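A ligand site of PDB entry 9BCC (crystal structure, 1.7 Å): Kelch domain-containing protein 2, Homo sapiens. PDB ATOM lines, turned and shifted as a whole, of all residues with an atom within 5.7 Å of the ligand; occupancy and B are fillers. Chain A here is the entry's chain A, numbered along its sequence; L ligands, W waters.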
ATOM      1  N   TYR A  38      26.958  17.609   5.559  1.00  0.00           N
ATOM      2  CA  TYR A  38      26.460  16.309   5.084  1.00  0.00           C
ATOM      3  C   TYR A  38      25.075  16.512   4.496  1.00  0.00           C
ATOM      4  O   TYR A  38      24.451  17.564   4.683  1.00  0.00           O
ATOM      5  CB  TYR A  38      26.411  15.262   6.225  1.00  0.00           C
ATOM      6  CG  TYR A  38      25.178  15.412   7.104  1.00  0.00           C
ATOM      7  CD1 TYR A  38      25.044  16.489   7.983  1.00  0.00           C
ATOM      8  CD2 TYR A  38      24.136  14.501   7.039  1.00  0.00           C
ATOM      9  CE1 TYR A  38      23.927  16.626   8.781  1.00  0.00           C
ATOM     10  CE2 TYR A  38      23.014  14.630   7.823  1.00  0.00           C
ATOM     11  CZ  TYR A  38      22.912  15.698   8.690  1.00  0.00           C
ATOM     12  OH  TYR A  38      21.781  15.842   9.461  1.00  0.00           O
ATOM     13  N   LYS A 135      30.044  20.692  16.918  1.00  0.00           N
ATOM     14  CA  LYS A 135      28.856  21.469  17.321  1.00  0.00           C
ATOM     15  C   LYS A 135      29.160  22.382  18.512  1.00  0.00           C
ATOM     16  O   LYS A 135      28.554  22.294  19.586  1.00  0.00           O
ATOM     17  CB  LYS A 135      27.679  20.529  17.594  1.00  0.00           C
ATOM     18  CG  LYS A 135      27.290  19.665  16.401  1.00  0.00           C
ATOM     19  CD  LYS A 135      25.969  18.890  16.664  1.00  0.00           C
ATOM     20  CE  LYS A 135      26.190  17.719  17.622  1.00  0.00           C
ATOM     21  NZ  LYS A 135      27.069  16.733  16.971  1.00  0.00           N
ATOM     22  N   TYR A 151      30.272  18.831  21.652  1.00  0.00           N
ATOM     23  CA  TYR A 151      29.892  17.422  21.844  1.00  0.00           C
ATOM     24  C   TYR A 151      31.012  16.525  21.368  1.00  0.00           C
ATOM     25  O   TYR A 151      31.455  16.673  20.227  1.00  0.00           O
ATOM     26  CB  TYR A 151      28.639  17.113  21.039  1.00  0.00           C
ATOM     27  CG  TYR A 151      27.941  15.801  21.357  1.00  0.00           C
ATOM     28  CD1 TYR A 151      27.288  15.608  22.574  1.00  0.00           C
ATOM     29  CD2 TYR A 151      27.886  14.787  20.418  1.00  0.00           C
ATOM     30  CE1 TYR A 151      26.623  14.410  22.847  1.00  0.00           C
ATOM     31  CE2 TYR A 151      27.219  13.593  20.682  1.00  0.00           C
ATOM     32  CZ  TYR A 151      26.605  13.412  21.906  1.00  0.00           C
ATOM     33  OH  TYR A 151      25.938  12.235  22.167  1.00  0.00           O
ATOM     34  N   ASP A 166      26.308  11.969  27.546  1.00  0.00           N
ATOM     35  CA  ASP A 166      24.972  11.832  26.967  1.00  0.00           C
ATOM     36  C   ASP A 166      24.625  10.345  27.013  1.00  0.00           C
ATOM     37  O   ASP A 166      25.088   9.558  26.198  1.00  0.00           O
ATOM     38  CB  ASP A 166      24.943  12.374  25.541  1.00  0.00           C
ATOM     39  CG  ASP A 166      23.618  12.120  24.825  1.00  0.00           C
ATOM     40  OD1 ASP A 166      22.652  11.597  25.434  1.00  0.00           O
ATOM     41  OD2 ASP A 166      23.536  12.451  23.630  1.00  0.00           O
ATOM     42  N   THR A 168      22.339   8.603  26.009  1.00  0.00           N
ATOM     43  CA  THR A 168      21.815   7.995  24.790  1.00  0.00           C
ATOM     44  C   THR A 168      22.910   7.423  23.906  1.00  0.00           C
ATOM     45  O   THR A 168      22.598   6.618  23.017  1.00  0.00           O
ATOM     46  CB  THR A 168      20.975   8.992  23.985  1.00  0.00           C
ATOM     47  OG1 THR A 168      21.815  10.047  23.488  1.00  0.00           O
ATOM     48  CG2 THR A 168      19.847   9.581  24.828  1.00  0.00           C
ATOM     49  N   ASN A 172      24.463   2.838  21.532  1.00  0.00           N
ATOM     50  CA  ASN A 172      24.352   2.834  20.073  1.00  0.00           C
ATOM     51  C   ASN A 172      25.678   3.063  19.360  1.00  0.00           C
ATOM     52  O   ASN A 172      25.692   3.282  18.145  1.00  0.00           O
ATOM     53  CB  ASN A 172      23.326   3.873  19.607  1.00  0.00           C
ATOM     54  CG  ASN A 172      23.641   5.283  20.111  1.00  0.00           C
ATOM     55  OD1 ASN A 172      24.791   5.607  20.428  1.00  0.00           O
ATOM     56  ND2 ASN A 172      22.619   6.130  20.176  1.00  0.00           N
ATOM     57  N   ARG A 177      29.863   9.606  24.240  1.00  0.00           N
ATOM     58  CA  ARG A 177      30.163  11.012  23.999  1.00  0.00           C
ATOM     59  C   ARG A 177      29.317  11.867  24.930  1.00  0.00           C
ATOM     60  O   ARG A 177      28.335  11.404  25.514  1.00  0.00           O
ATOM     61  CB  ARG A 177      29.925  11.386  22.534  1.00  0.00           C
ATOM     62  CG  ARG A 177      30.750  10.551  21.550  1.00  0.00           C
ATOM     63  CD  ARG A 177      30.669  11.093  20.148  1.00  0.00           C
ATOM     64  NE  ARG A 177      29.335  10.935  19.581  1.00  0.00           N
ATOM     65  CZ  ARG A 177      28.948  11.457  18.428  1.00  0.00           C
ATOM     66  NH1 ARG A 177      29.766  12.181  17.690  1.00  0.00           N
ATOM     67  NH2 ARG A 177      27.706  11.241  17.992  1.00  0.00           N
ATOM     68  N   TRP A 179      28.719  16.333  26.499  1.00  0.00           N
ATOM     69  CA  TRP A 179      28.801  17.782  26.389  1.00  0.00           C
ATOM     70  C   TRP A 179      29.834  18.353  27.361  1.00  0.00           C
ATOM     71  O   TRP A 179      30.012  17.850  28.474  1.00  0.00           O
ATOM     72  CB  TRP A 179      27.440  18.436  26.686  1.00  0.00           C
ATOM     73  CG  TRP A 179      26.308  17.933  25.839  1.00  0.00           C
ATOM     74  CD1 TRP A 179      25.973  18.331  24.569  1.00  0.00           C
ATOM     75  CD2 TRP A 179      25.327  16.951  26.213  1.00  0.00           C
ATOM     76  NE1 TRP A 179      24.857  17.652  24.134  1.00  0.00           N
ATOM     77  CE2 TRP A 179      24.438  16.794  25.116  1.00  0.00           C
ATOM     78  CE3 TRP A 179      25.118  16.175  27.363  1.00  0.00           C
ATOM     79  CZ2 TRP A 179      23.371  15.906  25.137  1.00  0.00           C
ATOM     80  CZ3 TRP A 179      24.045  15.294  27.388  1.00  0.00           C
ATOM     81  CH2 TRP A 179      23.189  15.162  26.272  1.00  0.00           C
ATOM     82  N   ALA A 207      26.036  21.714  23.503  1.00  0.00           N
ATOM     83  CA  ALA A 207      26.431  21.706  22.109  1.00  0.00           C
ATOM     84  C   ALA A 207      25.313  22.290  21.247  1.00  0.00           C
ATOM     85  O   ALA A 207      24.160  22.388  21.674  1.00  0.00           O
ATOM     86  CB  ALA A 207      26.780  20.283  21.635  1.00  0.00           C
ATOM     87  N   ALA A 208      25.672  22.684  20.028  1.00  0.00           N
ATOM     88  CA  ALA A 208      24.722  23.271  19.081  1.00  0.00           C
ATOM     89  C   ALA A 208      24.133  24.572  19.625  1.00  0.00           C
ATOM     90  O   ALA A 208      23.035  24.987  19.212  1.00  0.00           O
ATOM     91  CB  ALA A 208      23.600  22.270  18.711  1.00  0.00           C
ATOM     92  N   ARG A 224      21.876  22.577  23.276  1.00  0.00           N
ATOM     93  CA  ARG A 224      21.355  21.333  23.831  1.00  0.00           C
ATOM     94  C   ARG A 224      22.185  20.912  25.033  1.00  0.00           C
ATOM     95  O   ARG A 224      23.421  20.925  24.990  1.00  0.00           O
ATOM     96  CB  ARG A 224      21.387  20.213  22.787  1.00  0.00           C
ATOM     97  CG  ARG A 224      21.261  18.797  23.377  1.00  0.00           C
ATOM     98  CD  ARG A 224      19.815  18.334  23.477  1.00  0.00           C
ATOM     99  NE  ARG A 224      19.744  17.051  24.172  1.00  0.00           N
ATOM    100  CZ  ARG A 224      20.062  15.884  23.623  1.00  0.00           C
ATOM    101  NH1 ARG A 224      20.389  15.784  22.350  1.00  0.00           N
ATOM    102  NH2 ARG A 224      20.071  14.790  24.387  1.00  0.00           N
ATOM    103  N   ARG A 229      16.622  21.797  25.180  1.00  0.00           N
ATOM    104  CA  ARG A 229      17.235  22.800  24.319  1.00  0.00           C
ATOM    105  C   ARG A 229      16.846  24.164  24.877  1.00  0.00           C
ATOM    106  O   ARG A 229      15.663  24.427  25.128  1.00  0.00           O
ATOM    107  CB  ARG A 229      16.804  22.621  22.871  1.00  0.00           C
ATOM    108  CG  ARG A 229      17.384  21.320  22.295  1.00  0.00           C
ATOM    109  CD  ARG A 229      16.810  20.934  20.943  1.00  0.00           C
ATOM    110  NE  ARG A 229      17.396  19.655  20.535  1.00  0.00           N
ATOM    111  CZ  ARG A 229      16.755  18.493  20.524  1.00  0.00           C
ATOM    112  NH1 ARG A 229      15.442  18.413  20.725  1.00  0.00           N
ATOM    113  NH2 ARG A 229      17.449  17.382  20.314  1.00  0.00           N
ATOM    114  N   SER A 257      18.200  24.633  19.942  1.00  0.00           N
ATOM    115  CA  SER A 257      19.570  24.394  19.486  1.00  0.00           C
ATOM    116  C   SER A 257      19.595  24.534  17.970  1.00  0.00           C
ATOM    117  O   SER A 257      18.543  24.679  17.328  1.00  0.00           O
ATOM    118  CB  SER A 257      20.067  23.003  19.851  1.00  0.00           C
ATOM    119  OG  SER A 257      19.335  22.042  19.108  1.00  0.00           O
ATOM    120  N   TRP A 258      20.788  24.469  17.391  1.00  0.00           N
ATOM    121  CA  TRP A 258      20.987  24.464  15.934  1.00  0.00           C
ATOM    122  C   TRP A 258      20.458  25.735  15.259  1.00  0.00           C
ATOM    123  O   TRP A 258      20.128  25.724  14.067  1.00  0.00           O
ATOM    124  CB  TRP A 258      20.357  23.192  15.346  1.00  0.00           C
ATOM    125  CG  TRP A 258      21.336  22.018  15.354  1.00  0.00           C
ATOM    126  CD1 TRP A 258      22.662  22.069  15.124  1.00  0.00           C
ATOM    127  CD2 TRP A 258      21.033  20.630  15.627  1.00  0.00           C
ATOM    128  NE1 TRP A 258      23.223  20.798  15.190  1.00  0.00           N
ATOM    129  CE2 TRP A 258      22.232  19.904  15.506  1.00  0.00           C
ATOM    130  CE3 TRP A 258      19.852  19.946  15.942  1.00  0.00           C
ATOM    131  CZ2 TRP A 258      22.299  18.529  15.704  1.00  0.00           C
ATOM    132  CZ3 TRP A 258      19.919  18.571  16.140  1.00  0.00           C
ATOM    133  CH2 TRP A 258      21.135  17.873  16.017  1.00  0.00           C
ATOM    134  N   PHE A 275      15.777  24.539  16.654  1.00  0.00           N
ATOM    135  CA  PHE A 275      15.092  23.283  16.926  1.00  0.00           C
ATOM    136  C   PHE A 275      14.710  23.264  18.396  1.00  0.00           C
ATOM    137  O   PHE A 275      15.587  23.419  19.245  1.00  0.00           O
ATOM    138  CB  PHE A 275      16.046  22.121  16.583  1.00  0.00           C
ATOM    139  CG  PHE A 275      15.410  20.784  16.431  1.00  0.00           C
ATOM    140  CD1 PHE A 275      14.252  20.609  15.688  1.00  0.00           C
ATOM    141  CD2 PHE A 275      16.019  19.674  17.003  1.00  0.00           C
ATOM    142  CE1 PHE A 275      13.695  19.352  15.531  1.00  0.00           C
ATOM    143  CE2 PHE A 275      15.468  18.420  16.869  1.00  0.00           C
ATOM    144  CZ  PHE A 275      14.297  18.247  16.130  1.00  0.00           C
ATOM    145  N   TRP A 309      20.601  23.909  11.849  1.00  0.00           N
ATOM    146  CA  TRP A 309      21.958  23.549  11.430  1.00  0.00           C
ATOM    147  C   TRP A 309      22.326  24.213  10.120  1.00  0.00           C
ATOM    148  O   TRP A 309      23.193  23.730   9.392  1.00  0.00           O
ATOM    149  CB  TRP A 309      22.157  22.029  11.334  1.00  0.00           C
ATOM    150  CG  TRP A 309      23.483  21.572  11.886  1.00  0.00           C
ATOM    151  CD1 TRP A 309      24.502  22.361  12.363  1.00  0.00           C
ATOM    152  CD2 TRP A 309      23.941  20.213  12.027  1.00  0.00           C
ATOM    153  NE1 TRP A 309      25.547  21.585  12.824  1.00  0.00           N
ATOM    154  CE2 TRP A 309      25.239  20.267  12.599  1.00  0.00           C
ATOM    155  CE3 TRP A 309      23.391  18.964  11.714  1.00  0.00           C
ATOM    156  CZ2 TRP A 309      25.974  19.124  12.874  1.00  0.00           C
ATOM    157  CZ3 TRP A 309      24.134  17.827  11.990  1.00  0.00           C
ATOM    158  CH2 TRP A 309      25.419  17.916  12.560  1.00  0.00           C
ATOM    159  N   LEU A 330      15.986  16.681  11.276  1.00  0.00           N
ATOM    160  CA  LEU A 330      17.058  15.981  10.576  1.00  0.00           C
ATOM    161  C   LEU A 330      17.406  14.656  11.226  1.00  0.00           C
ATOM    162  O   LEU A 330      18.103  13.846  10.614  1.00  0.00           O
ATOM    163  CB  LEU A 330      18.299  16.875  10.492  1.00  0.00           C
ATOM    164  CG  LEU A 330      18.947  17.444  11.764  1.00  0.00           C
ATOM    165  CD1 LEU A 330      19.846  16.417  12.427  1.00  0.00           C
ATOM    166  CD2 LEU A 330      19.729  18.740  11.463  1.00  0.00           C
ATOM    167  N   LEU A 331      16.963  14.427  12.465  1.00  0.00           N
ATOM    168  CA  LEU A 331      17.246  13.170  13.151  1.00  0.00           C
ATOM    169  C   LEU A 331      16.523  11.998  12.498  1.00  0.00           C
ATOM    170  O   LEU A 331      16.924  10.860  12.713  1.00  0.00           O
ATOM    171  CB  LEU A 331      16.848  13.273  14.637  1.00  0.00           C
ATOM    172  CG  LEU A 331      17.452  14.478  15.380  1.00  0.00           C
ATOM    173  CD1 LEU A 331      16.821  14.624  16.762  1.00  0.00           C
ATOM    174  CD2 LEU A 331      18.943  14.275  15.488  1.00  0.00           C
ATOM    175  N   VAL A 332      15.467  12.247  11.737  1.00  0.00           N
ATOM    176  CA  VAL A 332      14.839  11.187  10.920  1.00  0.00           C
ATOM    177  C   VAL A 332      15.524  11.269   9.563  1.00  0.00           C
ATOM    178  O   VAL A 332      15.057  11.894   8.614  1.00  0.00           O
ATOM    179  CB  VAL A 332      13.320  11.341  10.830  1.00  0.00           C
ATOM    180  CG1 VAL A 332      12.721  10.146  10.079  1.00  0.00           C
ATOM    181  CG2 VAL A 332      12.704  11.482  12.218  1.00  0.00           C
ATOM    182  N   HIS A 333      16.694  10.631   9.468  1.00  0.00           N
ATOM    183  CA  HIS A 333      17.613  10.922   8.377  1.00  0.00           C
ATOM    184  C   HIS A 333      16.978  10.619   7.023  1.00  0.00           C
ATOM    185  O   HIS A 333      17.119  11.395   6.072  1.00  0.00           O
ATOM    186  CB  HIS A 333      18.925  10.153   8.581  1.00  0.00           C
ATOM    187  CG  HIS A 333      19.997  10.459   7.583  1.00  0.00           C
ATOM    188  ND1 HIS A 333      20.604  11.699   7.481  1.00  0.00           N
ATOM    189  CD2 HIS A 333      20.589   9.680   6.650  1.00  0.00           C
ATOM    190  CE1 HIS A 333      21.513  11.663   6.522  1.00  0.00           C
ATOM    191  NE2 HIS A 333      21.527  10.450   6.005  1.00  0.00           N
HETATM  192  C1  LIG L   1      23.325  13.509  20.226  1.00  0.00           C
HETATM  193  C2  LIG L   1      22.803  13.855  16.270  1.00  0.00           C
HETATM  194  C3  LIG L   1      23.058  14.867  14.110  1.00  0.00           C
HETATM  195  C4  LIG L   1      22.083  13.760  12.158  1.00  0.00           C
HETATM  196  C5  LIG L   1      21.112  11.738  13.796  1.00  0.00           C
HETATM  197  C6  LIG L   1      19.673   9.904  14.168  1.00  0.00           C
HETATM  198  C7  LIG L   1      21.860  12.787  14.340  1.00  0.00           C
HETATM  199  C8  LIG L   1      23.746  17.190  20.581  1.00  0.00           C
HETATM  200  C9  LIG L   1      22.236  18.798  19.382  1.00  0.00           C
HETATM  201  C10 LIG L   1      20.777  18.591  19.753  1.00  0.00           C
HETATM  202  C11 LIG L   1      24.417  15.823  20.620  1.00  0.00           C
HETATM  203  C12 LIG L   1      23.776  14.756  19.735  1.00  0.00           C
HETATM  204  C13 LIG L   1      23.063  13.891  17.752  1.00  0.00           C
HETATM  205  C14 LIG L   1      23.288  14.873  15.472  1.00  0.00           C
HETATM  206  C15 LIG L   1      22.329  13.794  13.539  1.00  0.00           C
HETATM  207  C16 LIG L   1      21.349  12.709  11.610  1.00  0.00           C
HETATM  208  C17 LIG L   1      20.861  11.694  12.423  1.00  0.00           C
HETATM  209  C18 LIG L   1      19.252   9.038  15.352  1.00  0.00           C
HETATM  210  C19 LIG L   1      20.938   7.462  14.924  1.00  0.00           C
HETATM  211  C20 LIG L   1      22.082  12.803  15.719  1.00  0.00           C
HETATM  212  N1  LIG L   1      22.906  17.512  19.471  1.00  0.00           N
HETATM  213  N2  LIG L   1      23.630  14.904  18.392  1.00  0.00           N
HETATM  214  O1  LIG L   1      23.909  17.981  21.444  1.00  0.00           O
HETATM  215  O2  LIG L   1      20.000  19.586  19.758  1.00  0.00           O
HETATM  216  O3  LIG L   1      20.344  17.446  20.048  1.00  0.00           O
HETATM  217  O4  LIG L   1      20.659  10.751  14.670  1.00  0.00           O
HETATM  218  O5  LIG L   1      20.408   8.398  15.826  1.00  0.00           O
HETATM  219  S1  LIG L   1      22.732  12.671  18.882  1.00  0.00           S
HETATM  220  O   HOH W   1      20.231  14.910  18.862  1.00  0.00           O
HETATM  221  O   HOH W   2      20.915  12.962  22.693  1.00  0.00           O
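An oxygen (O2) of the ligand lies within hydrogen-bond range of the side-chain hydroxyl of Ser 257, at 2.6 Å. The guanidinium group (NE) of Arg 229 lies within salt-bridge range of an oxygen (O2) of the ligand (2.7 Å). The guanidinium group of Arg 224 is in salt-bridge range of an oxygen (O3) of the ligand. NE1 of Trp 179 is in hydrogen-bond range of O1 of the ligand.
NE of Arg 229 lies close to OG of Ser 257, at 3.4 Å. The backbone NH (N) of Arg 224 is in hydrogen-bond range of the backbone carbonyl oxygen (O) of Ala 207, at 2.8 Å. OD2 of Asp 166 lies within hydrogen-bond range of OH of Tyr 151, at 2.8 Å. The side-chain carboxylate (OD1) of Asp 166 sits at hydrogen-bond distance from the side-chain hydroxyl (OG1) of Thr 168. N of Asp 166 is in hydrogen-bond range of O of Arg 177 (2.9 Å). N of Trp 258 is in hydrogen-bond range of O of Ala 208. O of Trp 258 is in hydrogen-bond range of N of Trp 309 (2.9 Å). O of Lys 135 is in hydrogen-bond range of N of Ala 208 (2.9 Å).
Residues that only touch the ligand: Leu 331 (3.3 Å), Tyr 38 (3.4 Å), Tyr 151 (3.4 Å), Leu 330 (3.5 Å), Asp 166 (3.6 Å), Trp 258 (3.7 Å), Ala 207 (3.7 Å), Lys 135 (3.8 Å), Ala 208 (3.8 Å) and Trp 309 (3.8 Å). Hydrophobic or aromatic side chains that line the ligand: Tyr 151, Trp 179, Ala 207, Ala 208, Trp 258, Trp 309, Leu 330 and Leu 331.
Water W2 lies within hydrogen-bond range of NH2 of Arg 224 (2.6 Å), OD2 of Asp 166 (2.8 Å) and OG1 of Thr 168 (3.2 Å).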
